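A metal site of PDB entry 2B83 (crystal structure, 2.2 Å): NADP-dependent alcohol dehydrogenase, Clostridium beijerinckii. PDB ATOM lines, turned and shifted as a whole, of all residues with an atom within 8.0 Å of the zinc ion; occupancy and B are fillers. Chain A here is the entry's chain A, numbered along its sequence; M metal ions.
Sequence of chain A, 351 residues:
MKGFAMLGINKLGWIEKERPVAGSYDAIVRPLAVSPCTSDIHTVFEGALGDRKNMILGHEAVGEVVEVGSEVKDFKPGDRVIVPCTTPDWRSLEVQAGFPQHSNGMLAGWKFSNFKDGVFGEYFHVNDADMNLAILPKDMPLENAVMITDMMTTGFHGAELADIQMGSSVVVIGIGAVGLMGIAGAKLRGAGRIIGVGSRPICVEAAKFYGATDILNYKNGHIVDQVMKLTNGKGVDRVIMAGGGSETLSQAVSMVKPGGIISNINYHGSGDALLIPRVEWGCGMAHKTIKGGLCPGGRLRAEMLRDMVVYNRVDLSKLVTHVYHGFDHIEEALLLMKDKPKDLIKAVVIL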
ATOM      1  N   SER A  35      28.526   9.201 -24.161  1.00  0.00           N
ATOM      2  CA  SER A  35      28.638   9.262 -22.713  1.00  0.00           C
ATOM      3  C   SER A  35      27.492  10.068 -22.096  1.00  0.00           C
ATOM      4  O   SER A  35      27.184  11.159 -22.555  1.00  0.00           O
ATOM      5  CB  SER A  35      29.966   9.887 -22.308  1.00  0.00           C
ATOM      6  OG  SER A  35      30.053  10.015 -20.898  1.00  0.00           O
ATOM      7  N   PRO A  36      26.841   9.518 -21.057  1.00  0.00           N
ATOM      8  CA  PRO A  36      25.744  10.231 -20.407  1.00  0.00           C
ATOM      9  C   PRO A  36      26.330  11.335 -19.527  1.00  0.00           C
ATOM     10  O   PRO A  36      27.474  11.232 -19.061  1.00  0.00           O
ATOM     11  CB  PRO A  36      25.043   9.137 -19.607  1.00  0.00           C
ATOM     12  CG  PRO A  36      26.206   8.280 -19.177  1.00  0.00           C
ATOM     13  CD  PRO A  36      27.033   8.184 -20.454  1.00  0.00           C
ATOM     14  N   CYS A  37      25.562  12.401 -19.301  1.00  0.00           N
ATOM     15  CA  CYS A  37      26.052  13.519 -18.496  1.00  0.00           C
ATOM     16  C   CYS A  37      25.093  13.911 -17.376  1.00  0.00           C
ATOM     17  O   CYS A  37      23.901  13.598 -17.425  1.00  0.00           O
ATOM     18  CB  CYS A  37      26.303  14.730 -19.399  1.00  0.00           C
ATOM     19  SG  CYS A  37      26.834  16.231 -18.525  1.00  0.00           S
ATOM     20  N   THR A  38      25.614  14.609 -16.376  1.00  0.00           N
ATOM     21  CA  THR A  38      24.781  15.063 -15.275  1.00  0.00           C
ATOM     22  C   THR A  38      23.711  16.003 -15.835  1.00  0.00           C
ATOM     23  O   THR A  38      22.619  16.129 -15.286  1.00  0.00           O
ATOM     24  CB  THR A  38      25.613  15.846 -14.238  1.00  0.00           C
ATOM     25  OG1 THR A  38      26.202  16.991 -14.869  1.00  0.00           O
ATOM     26  CG2 THR A  38      26.708  14.964 -13.684  1.00  0.00           C
ATOM     27  N   SER A  39      24.044  16.661 -16.950  1.00  0.00           N
ATOM     28  CA  SER A  39      23.105  17.576 -17.601  1.00  0.00           C
ATOM     29  C   SER A  39      21.866  16.815 -18.041  1.00  0.00           C
ATOM     30  O   SER A  39      20.748  17.339 -17.958  1.00  0.00           O
ATOM     31  CB  SER A  39      23.748  18.247 -18.818  1.00  0.00           C
ATOM     32  OG  SER A  39      24.738  19.179 -18.415  1.00  0.00           O
ATOM     33  N   ASP A  40      22.047  15.590 -18.512  1.00  0.00           N
ATOM     34  CA  ASP A  40      20.927  14.760 -18.941  1.00  0.00           C
ATOM     35  C   ASP A  40      20.021  14.530 -17.732  1.00  0.00           C
ATOM     36  O   ASP A  40      18.796  14.557 -17.850  1.00  0.00           O
ATOM     37  CB  ASP A  40      21.420  13.399 -19.455  1.00  0.00           C
ATOM     38  CG  ASP A  40      22.055  13.478 -20.848  1.00  0.00           C
ATOM     39  OD1 ASP A  40      21.364  13.940 -21.780  1.00  0.00           O
ATOM     40  OD2 ASP A  40      23.236  13.071 -21.003  1.00  0.00           O
ATOM     41  N   GLY A  58      21.459  12.825 -24.707  1.00  0.00           N
ATOM     42  CA  GLY A  58      22.873  12.712 -25.028  1.00  0.00           C
ATOM     43  C   GLY A  58      23.457  13.815 -25.895  1.00  0.00           C
ATOM     44  O   GLY A  58      22.857  14.229 -26.884  1.00  0.00           O
ATOM     45  N   HIS A  59      24.629  14.310 -25.508  1.00  0.00           N
ATOM     46  CA  HIS A  59      25.303  15.355 -26.289  1.00  0.00           C
ATOM     47  C   HIS A  59      26.816  15.191 -26.268  1.00  0.00           C
ATOM     48  O   HIS A  59      27.558  16.130 -26.525  1.00  0.00           O
ATOM     49  CB  HIS A  59      24.928  16.739 -25.763  1.00  0.00           C
ATOM     50  CG  HIS A  59      25.117  16.897 -24.289  1.00  0.00           C
ATOM     51  ND1 HIS A  59      24.127  16.577 -23.383  1.00  0.00           N
ATOM     52  CD2 HIS A  59      26.180  17.315 -23.567  1.00  0.00           C
ATOM     53  CE1 HIS A  59      24.585  16.785 -22.158  1.00  0.00           C
ATOM     54  NE2 HIS A  59      25.824  17.226 -22.242  1.00  0.00           N
ATOM     55  N   GLU A  60      27.260  13.984 -25.949  1.00  0.00           N
ATOM     56  CA  GLU A  60      28.676  13.677 -25.903  1.00  0.00           C
ATOM     57  C   GLU A  60      28.920  12.482 -26.806  1.00  0.00           C
ATOM     58  O   GLU A  60      28.567  11.350 -26.466  1.00  0.00           O
ATOM     59  CB  GLU A  60      29.106  13.351 -24.473  1.00  0.00           C
ATOM     60  CG  GLU A  60      29.183  14.570 -23.577  1.00  0.00           C
ATOM     61  CD  GLU A  60      29.443  14.215 -22.122  1.00  0.00           C
ATOM     62  OE1 GLU A  60      30.446  13.531 -21.826  1.00  0.00           O
ATOM     63  OE2 GLU A  60      28.643  14.643 -21.261  1.00  0.00           O
ATOM     64  N   CYS A  85      29.917  19.175 -27.967  1.00  0.00           N
ATOM     65  CA  CYS A  85      28.555  19.221 -27.452  1.00  0.00           C
ATOM     66  C   CYS A  85      27.873  20.529 -27.854  1.00  0.00           C
ATOM     67  O   CYS A  85      26.657  20.583 -27.996  1.00  0.00           O
ATOM     68  CB  CYS A  85      28.537  19.043 -25.932  1.00  0.00           C
ATOM     69  SG  CYS A  85      29.281  20.389 -24.978  1.00  0.00           S
ATOM     70  N   TRP A 110      24.148  25.280 -27.639  1.00  0.00           N
ATOM     71  CA  TRP A 110      24.138  23.893 -27.203  1.00  0.00           C
ATOM     72  C   TRP A 110      22.769  23.351 -27.592  1.00  0.00           C
ATOM     73  O   TRP A 110      21.761  23.644 -26.949  1.00  0.00           O
ATOM     74  CB  TRP A 110      24.373  23.801 -25.690  1.00  0.00           C
ATOM     75  CG  TRP A 110      23.982  22.481 -25.129  1.00  0.00           C
ATOM     76  CD1 TRP A 110      24.220  21.246 -25.660  1.00  0.00           C
ATOM     77  CD2 TRP A 110      23.209  22.263 -23.940  1.00  0.00           C
ATOM     78  NE1 TRP A 110      23.649  20.278 -24.886  1.00  0.00           N
ATOM     79  CE2 TRP A 110      23.015  20.868 -23.815  1.00  0.00           C
ATOM     80  CE3 TRP A 110      22.665  23.103 -22.961  1.00  0.00           C
ATOM     81  CZ2 TRP A 110      22.304  20.297 -22.764  1.00  0.00           C
ATOM     82  CZ3 TRP A 110      21.953  22.541 -21.908  1.00  0.00           C
ATOM     83  CH2 TRP A 110      21.772  21.146 -21.823  1.00  0.00           C
ATOM     84  N   PHE A 112      22.072  19.636 -28.873  1.00  0.00           N
ATOM     85  CA  PHE A 112      21.863  18.246 -28.449  1.00  0.00           C
ATOM     86  C   PHE A 112      21.286  18.089 -27.040  1.00  0.00           C
ATOM     87  O   PHE A 112      21.855  18.562 -26.068  1.00  0.00           O
ATOM     88  CB  PHE A 112      23.182  17.459 -28.528  1.00  0.00           C
ATOM     89  CG  PHE A 112      23.724  17.300 -29.928  1.00  0.00           C
ATOM     90  CD1 PHE A 112      22.903  16.858 -30.960  1.00  0.00           C
ATOM     91  CD2 PHE A 112      25.072  17.547 -30.193  1.00  0.00           C
ATOM     92  CE1 PHE A 112      23.419  16.672 -32.255  1.00  0.00           C
ATOM     93  CE2 PHE A 112      25.595  17.370 -31.475  1.00  0.00           C
ATOM     94  CZ  PHE A 112      24.764  16.927 -32.508  1.00  0.00           C
ATOM     95  N   SER A 113      20.157  17.384 -26.958  1.00  0.00           N
ATOM     96  CA  SER A 113      19.453  17.130 -25.702  1.00  0.00           C
ATOM     97  C   SER A 113      19.080  18.399 -24.934  1.00  0.00           C
ATOM     98  O   SER A 113      18.878  18.374 -23.710  1.00  0.00           O
ATOM     99  CB  SER A 113      20.243  16.171 -24.793  1.00  0.00           C
ATOM    100  OG  SER A 113      21.467  16.712 -24.352  1.00  0.00           O
ATOM    101  N   VAL A 146      35.691  11.048 -26.450  1.00  0.00           N
ATOM    102  CA  VAL A 146      34.370  11.471 -25.981  1.00  0.00           C
ATOM    103  C   VAL A 146      34.480  12.489 -24.851  1.00  0.00           C
ATOM    104  O   VAL A 146      33.600  13.333 -24.672  1.00  0.00           O
ATOM    105  CB  VAL A 146      33.559  10.253 -25.483  1.00  0.00           C
ATOM    106  CG1 VAL A 146      32.190  10.716 -24.987  1.00  0.00           C
ATOM    107  CG2 VAL A 146      33.387   9.248 -26.613  1.00  0.00           C
ATOM    108  N   THR A 149      34.469  16.300 -26.056  1.00  0.00           N
ATOM    109  CA  THR A 149      33.209  16.920 -26.452  1.00  0.00           C
ATOM    110  C   THR A 149      32.516  17.789 -25.414  1.00  0.00           C
ATOM    111  O   THR A 149      31.793  18.722 -25.781  1.00  0.00           O
ATOM    112  CB  THR A 149      32.203  15.854 -26.958  1.00  0.00           C
ATOM    113  OG1 THR A 149      31.712  15.084 -25.857  1.00  0.00           O
ATOM    114  CG2 THR A 149      32.880  14.938 -27.977  1.00  0.00           C
ATOM    115  N   ASP A 150      32.722  17.505 -24.131  1.00  0.00           N
ATOM    116  CA  ASP A 150      32.096  18.311 -23.093  1.00  0.00           C
ATOM    117  C   ASP A 150      32.925  18.507 -21.829  1.00  0.00           C
ATOM    118  O   ASP A 150      33.174  19.637 -21.415  1.00  0.00           O
ATOM    119  CB  ASP A 150      30.724  17.744 -22.707  1.00  0.00           C
ATOM    120  CG  ASP A 150      29.973  18.640 -21.738  1.00  0.00           C
ATOM    121  OD1 ASP A 150      30.387  19.807 -21.532  1.00  0.00           O
ATOM    122  OD2 ASP A 150      28.955  18.209 -21.187  1.00  0.00           O
ATOM    123  N   MET A 151      33.363  17.411 -21.219  1.00  0.00           N
ATOM    124  CA  MET A 151      34.148  17.496 -19.992  1.00  0.00           C
ATOM    125  C   MET A 151      35.383  18.374 -20.142  1.00  0.00           C
ATOM    126  O   MET A 151      35.543  19.355 -19.428  1.00  0.00           O
ATOM    127  CB  MET A 151      34.562  16.087 -19.526  1.00  0.00           C
ATOM    128  CG  MET A 151      33.376  15.176 -19.196  1.00  0.00           C
ATOM    129  SD  MET A 151      32.290  15.842 -17.899  1.00  0.00           S
ATOM    130  CE  MET A 151      30.966  16.597 -18.906  1.00  0.00           C
ATOM    131  N   THR A 154      34.488  22.106 -21.190  1.00  0.00           N
ATOM    132  CA  THR A 154      33.829  22.812 -20.095  1.00  0.00           C
ATOM    133  C   THR A 154      34.801  23.072 -18.941  1.00  0.00           C
ATOM    134  O   THR A 154      34.882  24.189 -18.427  1.00  0.00           O
ATOM    135  CB  THR A 154      32.634  21.999 -19.558  1.00  0.00           C
ATOM    136  OG1 THR A 154      31.658  21.859 -20.603  1.00  0.00           O
ATOM    137  CG2 THR A 154      31.987  22.708 -18.379  1.00  0.00           C
ATOM    138  N   VAL A 178      33.770  17.324 -14.508  1.00  0.00           N
ATOM    139  CA  VAL A 178      33.954  18.754 -14.801  1.00  0.00           C
ATOM    140  C   VAL A 178      35.016  19.404 -13.913  1.00  0.00           C
ATOM    141  O   VAL A 178      35.884  20.121 -14.398  1.00  0.00           O
ATOM    142  CB  VAL A 178      32.622  19.515 -14.657  1.00  0.00           C
ATOM    143  CG1 VAL A 178      32.851  21.014 -14.859  1.00  0.00           C
ATOM    144  CG2 VAL A 178      31.625  19.003 -15.664  1.00  0.00           C
ATOM    145  N   TYR A 267      26.281  23.529 -13.942  1.00  0.00           N
ATOM    146  CA  TYR A 267      24.934  23.705 -14.486  1.00  0.00           C
ATOM    147  C   TYR A 267      24.004  23.688 -13.271  1.00  0.00           C
ATOM    148  O   TYR A 267      23.590  22.634 -12.805  1.00  0.00           O
ATOM    149  CB  TYR A 267      24.623  22.539 -15.435  1.00  0.00           C
ATOM    150  CG  TYR A 267      23.217  22.456 -16.009  1.00  0.00           C
ATOM    151  CD1 TYR A 267      22.150  23.150 -15.444  1.00  0.00           C
ATOM    152  CD2 TYR A 267      22.952  21.602 -17.081  1.00  0.00           C
ATOM    153  CE1 TYR A 267      20.846  22.989 -15.927  1.00  0.00           C
ATOM    154  CE2 TYR A 267      21.660  21.434 -17.575  1.00  0.00           C
ATOM    155  CZ  TYR A 267      20.621  22.127 -16.987  1.00  0.00           C
ATOM    156  OH  TYR A 267      19.341  21.927 -17.468  1.00  0.00           O
ATOM    157  N   CYS A 295      30.178  25.963 -22.157  1.00  0.00           N
ATOM    158  CA  CYS A 295      31.442  25.645 -22.811  1.00  0.00           C
ATOM    159  C   CYS A 295      31.483  26.035 -24.291  1.00  0.00           C
ATOM    160  O   CYS A 295      30.479  25.971 -24.992  1.00  0.00           O
ATOM    161  CB  CYS A 295      31.726  24.154 -22.710  1.00  0.00           C
ATOM    162  SG  CYS A 295      30.529  23.107 -23.613  1.00  0.00           S
ATOM    163  N   MET A 337      24.527   7.596 -13.845  1.00  0.00           N
ATOM    164  CA  MET A 337      24.777   9.007 -13.583  1.00  0.00           C
ATOM    165  C   MET A 337      23.732   9.553 -12.608  1.00  0.00           C
ATOM    166  O   MET A 337      23.973  10.549 -11.917  1.00  0.00           O
ATOM    167  CB  MET A 337      24.735   9.811 -14.883  1.00  0.00           C
ATOM    168  CG  MET A 337      25.888   9.532 -15.832  1.00  0.00           C
ATOM    169  SD  MET A 337      27.488   9.913 -15.086  1.00  0.00           S
ATOM    170  CE  MET A 337      27.496  11.709 -15.225  1.00  0.00           C
ATOM    171  N   LYS A 346      33.171   9.087 -15.110  1.00  0.00           N
ATOM    172  CA  LYS A 346      32.427   9.120 -16.379  1.00  0.00           C
ATOM    173  C   LYS A 346      32.305   7.711 -16.951  1.00  0.00           C
ATOM    174  O   LYS A 346      33.174   6.855 -16.754  1.00  0.00           O
ATOM    175  CB  LYS A 346      33.108  10.035 -17.416  1.00  0.00           C
ATOM    176  CG  LYS A 346      32.963  11.536 -17.147  1.00  0.00           C
ATOM    177  CD  LYS A 346      31.537  12.065 -17.369  1.00  0.00           C
ATOM    178  CE  LYS A 346      31.232  12.307 -18.852  1.00  0.00           C
ATOM    179  NZ  LYS A 346      29.878  12.905 -19.064  1.00  0.00           N
HETATM  180 ZN    ZN M   1      27.573  16.874 -20.831  1.00  0.00          ZN
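Met 151 touches the zinc ion.
The zinc ion is bound by the side-chain carboxylate (OD2) of Asp 150 (2.0 Å), a ring nitrogen (NE2) of His 59 (2.3 Å), the side-chain sulfur (SG) of Cys 37 (2.5 Å) and the side-chain carboxylate (OE2) of Glu 60 (2.5 Å). The zinc ion has four donor atoms within binding distance.
N of Cys 37 sits at hydrogen-bond distance from OD2 of Asp 40 (3.0 Å). The side-chain hydroxyl (OG) of Ser 113 sits at hydrogen-bond distance from a ring nitrogen (ND1) of His 59 (2.8 Å). N of Ser 39 sits close to SG of Cys 37. N of Ser 35 lies within hydrogen-bond range of O of Glu 60 (3.2 Å). The side-chain carboxylate (OD1) of Asp 150 sits at hydrogen-bond distance from the side-chain sulfur (SG) of Cys 85 (3.7 Å). OG1 of Thr 154 sits at hydrogen-bond distance from OD1 of Asp 150. The side-chain sulfur (SG) of Cys 37 sits close to the side-chain hydroxyl (OG1) of Thr 38. The side-chain amino group (NZ) of Lys 346 lies within salt-bridge range of the side-chain carboxylate (OE1) of Glu 60, 2.9 Å away.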
